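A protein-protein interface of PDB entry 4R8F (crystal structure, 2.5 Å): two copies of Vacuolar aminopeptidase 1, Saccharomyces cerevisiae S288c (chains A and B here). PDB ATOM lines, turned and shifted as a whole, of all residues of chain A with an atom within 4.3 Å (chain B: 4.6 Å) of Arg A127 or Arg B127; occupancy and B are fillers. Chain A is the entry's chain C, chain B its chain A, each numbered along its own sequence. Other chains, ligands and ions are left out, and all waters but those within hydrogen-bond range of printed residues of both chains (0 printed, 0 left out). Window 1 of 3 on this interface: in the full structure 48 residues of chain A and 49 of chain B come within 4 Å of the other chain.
O of Asp B126 is in hydrogen-bond range of NH1 of Arg A127 (3.1 Å).
The backbone carbonyl oxygen (O) of Leu A125 lies within hydrogen-bond range of the guanidinium group (NH2) of Arg B127, at 2.9 Å.
NH2 of Arg B159 sits at hydrogen-bond distance from O of Arg A438 (2.6 Å).
The guanidinium group (NH1) of Arg B127 lies within hydrogen-bond range of the backbone carbonyl oxygen (O) of Asp A126, 2.9 Å away.
The guanidinium group (NE) of Arg B127 lies close to the guanidinium group (NH2) of Arg A127 (3.5 Å).
O of Leu B125 sits at hydrogen-bond distance from NH2 of Arg A127 (3.1 Å).
The guanidinium group (NH2) of Arg A159 lies within hydrogen-bond range of the backbone carbonyl oxygen (O) of Arg B438 (2.5 Å).
NH2 of Arg A438 lies within salt-bridge range of OD2 of Asp B128 (2.9 Å).
OD2 of Asp A128 lies within salt-bridge range of NH2 of Arg B438.
The backbone carbonyl oxygen (O) of Leu A123 lies within hydrogen-bond range of the guanidinium group (NE) of Arg A127 (2.9 Å).
OD1 of Asp B126 lies within salt-bridge range of NH2 of Arg B159, at 3.1 Å.
The backbone carbonyl oxygen (O) of Leu B123 lies within hydrogen-bond range of the guanidinium group (NE) of Arg B127.
OD1 of Asp A126 lies within salt-bridge range of NH2 of Arg A159 (3.5 Å).
Leu A123 touches Leu B125.
Asp B126 touches Leu A123.
Leu B123 touches Asp A126 (CD2 to OD2, 3.9 Å).
Asp A126 touches Arg B438 (CB to O, 3.5 Å).
CB of Asp B126 touches O of Arg A438, 3.5 Å away.
Of chain B, only Leu B125, Asp B126 and Arg B127 come within 4 Å of Arg A127.
Arg B127 touches three residues of chain A.
Of the printed residues of chain B, Leu A123 touches Leu B125 (3.6 Å) and Asp B126 (3.8 Å).
Of the printed residues of chain A, Asp B126 touches Leu A123 (3.8 Å), Arg A127 (3.1 Å) and Arg A438 (3.5 Å).
Leu B129 touches none of the printed residues of chain A.
The nearest printed residue of chain B that does not touch Arg A127 is Leu B123 (5.0 Å).
Hydrophobic or aromatic side chains of chain B within 4 Å of the printed part of chain A: Leu B123 and Leu B125.
Along chain B the printed residues that touch a printed residue of chain A span positions 123 to 438.
Of the 12 printed residues of chain A, 7 touch a printed residue of chain B.
Hydrophobic or aromatic side chains of chain A within 4 Å of the printed part of chain B: Leu A123.
Among the printed residues, Asp or Glu carboxylates within 4 Å of a Lys or Arg side-chain nitrogen of the other chain: Asp A128 with Arg B438 (2.9 Å) and Arg A438 with Asp B128 (2.9 Å).
Leu A123 touches Asp B126, and with the chains exchanged Asp A126 touches Leu B123.
Asp A126 touches Arg B127, and with the chains exchanged Arg A127 touches Asp B126.
Asp A126 touches Arg B438, and with the chains exchanged Arg A438 touches Asp B126.
Arg B127 touches its own counterpart, Arg A127.
Of the 14 pairs that touch across the chains among the printed residues, 13 have their exchanged pair printed and touching as well.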
ATOM      1  N   LEU A 123      16.344 -13.283   3.470  1.00  0.00           N
ATOM      2  CA  LEU A 123      17.632 -13.120   4.155  1.00  0.00           C
ATOM      3  C   LEU A 123      18.694 -12.413   3.306  1.00  0.00           C
ATOM      4  O   LEU A 123      19.706 -11.956   3.836  1.00  0.00           O
ATOM      5  CB  LEU A 123      18.172 -14.479   4.604  1.00  0.00           C
ATOM      6  CG  LEU A 123      17.282 -15.307   5.530  1.00  0.00           C
ATOM      7  CD1 LEU A 123      17.730 -16.761   5.556  1.00  0.00           C
ATOM      8  CD2 LEU A 123      17.289 -14.721   6.930  1.00  0.00           C
ATOM      9  N   TRP A 124      18.468 -12.331   1.999  1.00  0.00           N
ATOM     10  CA  TRP A 124      19.354 -11.591   1.104  1.00  0.00           C
ATOM     11  C   TRP A 124      19.003 -10.105   0.993  1.00  0.00           C
ATOM     12  O   TRP A 124      19.722  -9.345   0.341  1.00  0.00           O
ATOM     13  CB  TRP A 124      19.359 -12.253  -0.276  1.00  0.00           C
ATOM     14  CG  TRP A 124      20.111 -13.539  -0.236  1.00  0.00           C
ATOM     15  CD1 TRP A 124      19.737 -14.691   0.397  1.00  0.00           C
ATOM     16  CD2 TRP A 124      21.392 -13.795  -0.809  1.00  0.00           C
ATOM     17  NE1 TRP A 124      20.701 -15.650   0.242  1.00  0.00           N
ATOM     18  CE2 TRP A 124      21.731 -15.126  -0.496  1.00  0.00           C
ATOM     19  CE3 TRP A 124      22.286 -13.027  -1.562  1.00  0.00           C
ATOM     20  CZ2 TRP A 124      22.922 -15.711  -0.916  1.00  0.00           C
ATOM     21  CZ3 TRP A 124      23.475 -13.610  -1.979  1.00  0.00           C
ATOM     22  CH2 TRP A 124      23.780 -14.939  -1.657  1.00  0.00           C
ATOM     23  N   LEU A 125      17.911  -9.692   1.635  1.00  0.00           N
ATOM     24  CA  LEU A 125      17.500  -8.287   1.627  1.00  0.00           C
ATOM     25  C   LEU A 125      18.328  -7.458   2.612  1.00  0.00           C
ATOM     26  O   LEU A 125      18.656  -7.917   3.709  1.00  0.00           O
ATOM     27  CB  LEU A 125      16.013  -8.161   1.954  1.00  0.00           C
ATOM     28  CG  LEU A 125      15.070  -8.876   0.982  1.00  0.00           C
ATOM     29  CD1 LEU A 125      13.670  -8.998   1.566  1.00  0.00           C
ATOM     30  CD2 LEU A 125      15.033  -8.156  -0.357  1.00  0.00           C
ATOM     31  N   ASP A 126      18.672  -6.244   2.192  1.00  0.00           N
ATOM     32  CA  ASP A 126      19.421  -5.297   3.022  1.00  0.00           C
ATOM     33  C   ASP A 126      20.752  -5.872   3.510  1.00  0.00           C
ATOM     34  O   ASP A 126      21.067  -5.852   4.704  1.00  0.00           O
ATOM     35  CB  ASP A 126      18.552  -4.816   4.192  1.00  0.00           C
ATOM     36  CG  ASP A 126      17.229  -4.222   3.728  1.00  0.00           C
ATOM     37  OD1 ASP A 126      17.153  -3.743   2.576  1.00  0.00           O
ATOM     38  OD2 ASP A 126      16.264  -4.234   4.517  1.00  0.00           O
ATOM     39  N   ARG A 127      21.518  -6.392   2.556  1.00  0.00           N
ATOM     40  CA  ARG A 127      22.867  -6.881   2.796  1.00  0.00           C
ATOM     41  C   ARG A 127      23.807  -6.124   1.870  1.00  0.00           C
ATOM     42  O   ARG A 127      23.473  -5.877   0.715  1.00  0.00           O
ATOM     43  CB  ARG A 127      22.949  -8.379   2.516  1.00  0.00           C
ATOM     44  CG  ARG A 127      21.971  -9.230   3.321  1.00  0.00           C
ATOM     45  CD  ARG A 127      22.490  -9.544   4.715  1.00  0.00           C
ATOM     46  NE  ARG A 127      21.572 -10.406   5.458  1.00  0.00           N
ATOM     47  CZ  ARG A 127      21.847 -10.994   6.621  1.00  0.00           C
ATOM     48  NH1 ARG A 127      23.023 -10.828   7.209  1.00  0.00           N
ATOM     49  NH2 ARG A 127      20.935 -11.762   7.201  1.00  0.00           N
ATOM     50  N   ASP A 128      24.973  -5.747   2.381  1.00  0.00           N
ATOM     51  CA  ASP A 128      25.983  -5.065   1.584  1.00  0.00           C
ATOM     52  C   ASP A 128      26.556  -6.058   0.573  1.00  0.00           C
ATOM     53  O   ASP A 128      27.255  -6.997   0.953  1.00  0.00           O
ATOM     54  CB  ASP A 128      27.090  -4.514   2.490  1.00  0.00           C
ATOM     55  CG  ASP A 128      26.575  -3.491   3.505  1.00  0.00           C
ATOM     56  OD1 ASP A 128      25.349  -3.260   3.575  1.00  0.00           O
ATOM     57  OD2 ASP A 128      27.402  -2.919   4.244  1.00  0.00           O
ATOM     58  N   LEU A 129      26.241  -5.869  -0.707  1.00  0.00           N
ATOM     59  CA  LEU A 129      26.643  -6.823  -1.738  1.00  0.00           C
ATOM     60  C   LEU A 129      27.779  -6.306  -2.605  1.00  0.00           C
ATOM     61  O   LEU A 129      27.644  -5.279  -3.268  1.00  0.00           O
ATOM     62  CB  LEU A 129      25.457  -7.182  -2.629  1.00  0.00           C
ATOM     63  CG  LEU A 129      24.265  -7.842  -1.934  1.00  0.00           C
ATOM     64  CD1 LEU A 129      23.186  -8.170  -2.952  1.00  0.00           C
ATOM     65  CD2 LEU A 129      24.690  -9.096  -1.183  1.00  0.00           C
ATOM     66  N   CYS A 158      26.092  -2.669  -4.441  1.00  0.00           N
ATOM     67  CA  CYS A 158      24.644  -2.708  -4.526  1.00  0.00           C
ATOM     68  C   CYS A 158      23.993  -3.446  -3.366  1.00  0.00           C
ATOM     69  O   CYS A 158      24.666  -3.985  -2.485  1.00  0.00           O
ATOM     70  CB  CYS A 158      24.235  -3.360  -5.841  1.00  0.00           C
ATOM     71  SG  CYS A 158      24.476  -5.147  -5.853  1.00  0.00           S
ATOM     72  N   ARG A 159      22.666  -3.450  -3.384  1.00  0.00           N
ATOM     73  CA  ARG A 159      21.862  -4.019  -2.317  1.00  0.00           C
ATOM     74  C   ARG A 159      20.483  -4.302  -2.890  1.00  0.00           C
ATOM     75  O   ARG A 159      20.006  -3.559  -3.745  1.00  0.00           O
ATOM     76  CB  ARG A 159      21.824  -3.021  -1.150  1.00  0.00           C
ATOM     77  CG  ARG A 159      20.536  -2.911  -0.339  1.00  0.00           C
ATOM     78  CD  ARG A 159      20.368  -1.480   0.166  1.00  0.00           C
ATOM     79  NE  ARG A 159      19.667  -1.393   1.443  1.00  0.00           N
ATOM     80  CZ  ARG A 159      20.239  -1.542   2.636  1.00  0.00           C
ATOM     81  NH1 ARG A 159      21.541  -1.808   2.755  1.00  0.00           N
ATOM     82  NH2 ARG A 159      19.496  -1.437   3.727  1.00  0.00           N
ATOM     83  N   ASP A 239      27.668 -11.238  -0.273  1.00  0.00           N
ATOM     84  CA  ASP A 239      27.723 -10.494   0.978  1.00  0.00           C
ATOM     85  C   ASP A 239      29.168 -10.138   1.286  1.00  0.00           C
ATOM     86  O   ASP A 239      30.022 -11.007   1.403  1.00  0.00           O
ATOM     87  CB  ASP A 239      27.130 -11.303   2.135  1.00  0.00           C
ATOM     88  CG  ASP A 239      26.893 -10.458   3.388  1.00  0.00           C
ATOM     89  OD1 ASP A 239      27.522  -9.385   3.540  1.00  0.00           O
ATOM     90  OD2 ASP A 239      26.072 -10.875   4.235  1.00  0.00           O
ATOM     91  N   ILE A 437      22.340 -16.256   3.804  1.00  0.00           N
ATOM     92  CA  ILE A 437      23.460 -15.493   3.274  1.00  0.00           C
ATOM     93  C   ILE A 437      24.610 -15.450   4.287  1.00  0.00           C
ATOM     94  O   ILE A 437      25.746 -15.146   3.928  1.00  0.00           O
ATOM     95  CB  ILE A 437      23.017 -14.068   2.876  1.00  0.00           C
ATOM     96  CG1 ILE A 437      24.056 -13.425   1.957  1.00  0.00           C
ATOM     97  CG2 ILE A 437      22.748 -13.201   4.104  1.00  0.00           C
ATOM     98  CD1 ILE A 437      23.624 -12.090   1.390  1.00  0.00           C
ATOM     99  N   ARG A 438      24.304 -15.748   5.549  1.00  0.00           N
ATOM    100  CA  ARG A 438      25.298 -15.769   6.612  1.00  0.00           C
ATOM    101  C   ARG A 438      24.960 -16.891   7.585  1.00  0.00           C
ATOM    102  O   ARG A 438      24.031 -16.768   8.381  1.00  0.00           O
ATOM    103  CB  ARG A 438      25.308 -14.422   7.335  1.00  0.00           C
ATOM    104  CG  ARG A 438      26.528 -14.164   8.204  1.00  0.00           C
ATOM    105  CD  ARG A 438      26.529 -12.718   8.681  1.00  0.00           C
ATOM    106  NE  ARG A 438      27.695 -12.376   9.495  1.00  0.00           N
ATOM    107  CZ  ARG A 438      28.903 -12.082   9.016  1.00  0.00           C
ATOM    108  NH1 ARG A 438      29.145 -12.099   7.707  1.00  0.00           N
ATOM    109  NH2 ARG A 438      29.882 -11.772   9.861  1.00  0.00           N
ATOM    110  N   LEU B 123      14.270  -9.911   8.486  1.00  0.00           N
ATOM    111  CA  LEU B 123      15.463  -9.058   8.414  1.00  0.00           C
ATOM    112  C   LEU B 123      16.390  -9.119   9.644  1.00  0.00           C
ATOM    113  O   LEU B 123      17.585  -8.870   9.515  1.00  0.00           O
ATOM    114  CB  LEU B 123      15.046  -7.601   8.167  1.00  0.00           C
ATOM    115  CG  LEU B 123      14.682  -7.118   6.753  1.00  0.00           C
ATOM    116  CD1 LEU B 123      14.121  -8.205   5.855  1.00  0.00           C
ATOM    117  CD2 LEU B 123      13.688  -5.967   6.827  1.00  0.00           C
ATOM    118  N   TRP B 124      15.849  -9.429  10.821  1.00  0.00           N
ATOM    119  CA  TRP B 124      16.671  -9.609  12.033  1.00  0.00           C
ATOM    120  C   TRP B 124      17.343 -10.984  12.136  1.00  0.00           C
ATOM    121  O   TRP B 124      18.170 -11.206  13.022  1.00  0.00           O
ATOM    122  CB  TRP B 124      15.844  -9.349  13.307  1.00  0.00           C
ATOM    123  CG  TRP B 124      16.056  -7.987  13.882  1.00  0.00           C
ATOM    124  CD1 TRP B 124      16.816  -7.661  14.974  1.00  0.00           C
ATOM    125  CD2 TRP B 124      15.522  -6.762  13.384  1.00  0.00           C
ATOM    126  NE1 TRP B 124      16.777  -6.303  15.187  1.00  0.00           N
ATOM    127  CE2 TRP B 124      15.989  -5.728  14.224  1.00  0.00           C
ATOM    128  CE3 TRP B 124      14.691  -6.437  12.309  1.00  0.00           C
ATOM    129  CZ2 TRP B 124      15.653  -4.391  14.019  1.00  0.00           C
ATOM    130  CZ3 TRP B 124      14.353  -5.110  12.106  1.00  0.00           C
ATOM    131  CH2 TRP B 124      14.835  -4.100  12.958  1.00  0.00           C
ATOM    132  N   LEU B 125      16.991 -11.904  11.245  1.00  0.00           N
ATOM    133  CA  LEU B 125      17.562 -13.251  11.262  1.00  0.00           C
ATOM    134  C   LEU B 125      18.970 -13.273  10.672  1.00  0.00           C
ATOM    135  O   LEU B 125      19.249 -12.604   9.675  1.00  0.00           O
ATOM    136  CB  LEU B 125      16.670 -14.221  10.489  1.00  0.00           C
ATOM    137  CG  LEU B 125      15.244 -14.390  11.022  1.00  0.00           C
ATOM    138  CD1 LEU B 125      14.369 -15.064   9.978  1.00  0.00           C
ATOM    139  CD2 LEU B 125      15.242 -15.186  12.317  1.00  0.00           C
ATOM    140  N   ASP B 126      19.847 -14.048  11.304  1.00  0.00           N
ATOM    141  CA  ASP B 126      21.219 -14.239  10.838  1.00  0.00           C
ATOM    142  C   ASP B 126      21.965 -12.920  10.691  1.00  0.00           C
ATOM    143  O   ASP B 126      22.586 -12.649   9.658  1.00  0.00           O
ATOM    144  CB  ASP B 126      21.235 -15.021   9.521  1.00  0.00           C
ATOM    145  CG  ASP B 126      20.479 -16.339   9.613  1.00  0.00           C
ATOM    146  OD1 ASP B 126      20.361 -16.898  10.727  1.00  0.00           O
ATOM    147  OD2 ASP B 126      19.995 -16.814   8.566  1.00  0.00           O
ATOM    148  N   ARG B 127      21.881 -12.106  11.741  1.00  0.00           N
ATOM    149  CA  ARG B 127      22.641 -10.872  11.848  1.00  0.00           C
ATOM    150  C   ARG B 127      23.463 -10.963  13.129  1.00  0.00           C
ATOM    151  O   ARG B 127      22.996 -11.496  14.130  1.00  0.00           O
ATOM    152  CB  ARG B 127      21.703  -9.667  11.899  1.00  0.00           C
ATOM    153  CG  ARG B 127      20.734  -9.557  10.725  1.00  0.00           C
ATOM    154  CD  ARG B 127      21.299  -8.768   9.553  1.00  0.00           C
ATOM    155  NE  ARG B 127      20.307  -8.608   8.489  1.00  0.00           N
ATOM    156  CZ  ARG B 127      20.472  -7.868   7.390  1.00  0.00           C
ATOM    157  NH1 ARG B 127      21.596  -7.194   7.179  1.00  0.00           N
ATOM    158  NH2 ARG B 127      19.499  -7.796   6.492  1.00  0.00           N
ATOM    159  N   ASP B 128      24.692 -10.463  13.092  1.00  0.00           N
ATOM    160  CA  ASP B 128      25.565 -10.482  14.262  1.00  0.00           C
ATOM    161  C   ASP B 128      25.048  -9.451  15.270  1.00  0.00           C
ATOM    162  O   ASP B 128      24.965  -8.264  14.947  1.00  0.00           O
ATOM    163  CB  ASP B 128      27.005 -10.154  13.857  1.00  0.00           C
ATOM    164  CG  ASP B 128      27.559 -11.101  12.789  1.00  0.00           C
ATOM    165  OD1 ASP B 128      26.915 -12.124  12.477  1.00  0.00           O
ATOM    166  OD2 ASP B 128      28.647 -10.810  12.249  1.00  0.00           O
ATOM    167  N   LEU B 129      24.702  -9.896  16.480  1.00  0.00           N
ATOM    168  CA  LEU B 129      24.095  -9.009  17.474  1.00  0.00           C
ATOM    169  C   LEU B 129      24.946  -8.813  18.716  1.00  0.00           C
ATOM    170  O   LEU B 129      25.257  -9.763  19.428  1.00  0.00           O
ATOM    171  CB  LEU B 129      22.717  -9.524  17.892  1.00  0.00           C
ATOM    172  CG  LEU B 129      21.688  -9.723  16.778  1.00  0.00           C
ATOM    173  CD1 LEU B 129      20.410 -10.310  17.354  1.00  0.00           C
ATOM    174  CD2 LEU B 129      21.389  -8.429  16.040  1.00  0.00           C
ATOM    175  N   CYS B 158      25.501 -12.909  20.246  1.00  0.00           N
ATOM    176  CA  CYS B 158      24.369 -13.748  19.914  1.00  0.00           C
ATOM    177  C   CYS B 158      23.798 -13.477  18.529  1.00  0.00           C
ATOM    178  O   CYS B 158      24.250 -12.583  17.814  1.00  0.00           O
ATOM    179  CB  CYS B 158      23.277 -13.558  20.962  1.00  0.00           C
ATOM    180  SG  CYS B 158      22.158 -12.185  20.611  1.00  0.00           S
ATOM    181  N   ARG B 159      22.793 -14.271  18.168  1.00  0.00           N
ATOM    182  CA  ARG B 159      22.121 -14.156  16.880  1.00  0.00           C
ATOM    183  C   ARG B 159      20.792 -14.922  16.898  1.00  0.00           C
ATOM    184  O   ARG B 159      20.640 -15.893  17.634  1.00  0.00           O
ATOM    185  CB  ARG B 159      23.071 -14.644  15.777  1.00  0.00           C
ATOM    186  CG  ARG B 159      22.518 -15.621  14.752  1.00  0.00           C
ATOM    187  CD  ARG B 159      23.638 -16.523  14.263  1.00  0.00           C
ATOM    188  NE  ARG B 159      23.316 -17.193  13.007  1.00  0.00           N
ATOM    189  CZ  ARG B 159      23.791 -16.854  11.809  1.00  0.00           C
ATOM    190  NH1 ARG B 159      24.639 -15.835  11.656  1.00  0.00           N
ATOM    191  NH2 ARG B 159      23.417 -17.552  10.746  1.00  0.00           N
ATOM    192  N   ASP B 239      22.598  -4.796  15.881  1.00  0.00           N
ATOM    193  CA  ASP B 239      23.526  -5.189  14.822  1.00  0.00           C
ATOM    194  C   ASP B 239      24.885  -4.531  15.041  1.00  0.00           C
ATOM    195  O   ASP B 239      24.978  -3.314  15.105  1.00  0.00           O
ATOM    196  CB  ASP B 239      22.967  -4.784  13.447  1.00  0.00           C
ATOM    197  CG  ASP B 239      23.628  -5.530  12.289  1.00  0.00           C
ATOM    198  OD1 ASP B 239      24.733  -6.081  12.466  1.00  0.00           O
ATOM    199  OD2 ASP B 239      23.038  -5.560  11.186  1.00  0.00           O
ATOM    200  N   ILE B 437      16.770  -3.741   9.874  1.00  0.00           N
ATOM    201  CA  ILE B 437      17.907  -3.717  10.783  1.00  0.00           C
ATOM    202  C   ILE B 437      19.079  -2.955  10.157  1.00  0.00           C
ATOM    203  O   ILE B 437      19.951  -2.471  10.872  1.00  0.00           O
ATOM    204  CB  ILE B 437      18.336  -5.143  11.188  1.00  0.00           C
ATOM    205  CG1 ILE B 437      19.148  -5.099  12.489  1.00  0.00           C
ATOM    206  CG2 ILE B 437      19.092  -5.836  10.051  1.00  0.00           C
ATOM    207  CD1 ILE B 437      19.628  -6.452  12.965  1.00  0.00           C
ATOM    208  N   ARG B 438      19.094  -2.866   8.826  1.00  0.00           N
ATOM    209  CA  ARG B 438      20.079  -2.072   8.096  1.00  0.00           C
ATOM    210  C   ARG B 438      19.360  -1.314   6.986  1.00  0.00           C
ATOM    211  O   ARG B 438      18.780  -1.933   6.092  1.00  0.00           O
ATOM    212  CB  ARG B 438      21.159  -2.983   7.508  1.00  0.00           C
ATOM    213  CG  ARG B 438      22.471  -2.289   7.169  1.00  0.00           C
ATOM    214  CD  ARG B 438      23.515  -3.311   6.751  1.00  0.00           C
ATOM    215  NE  ARG B 438      24.807  -2.707   6.412  1.00  0.00           N
ATOM    216  CZ  ARG B 438      25.750  -2.368   7.291  1.00  0.00           C
ATOM    217  NH1 ARG B 438      25.570  -2.547   8.599  1.00  0.00           N
ATOM    218  NH2 ARG B 438      26.889  -1.838   6.857  1.00  0.00           N
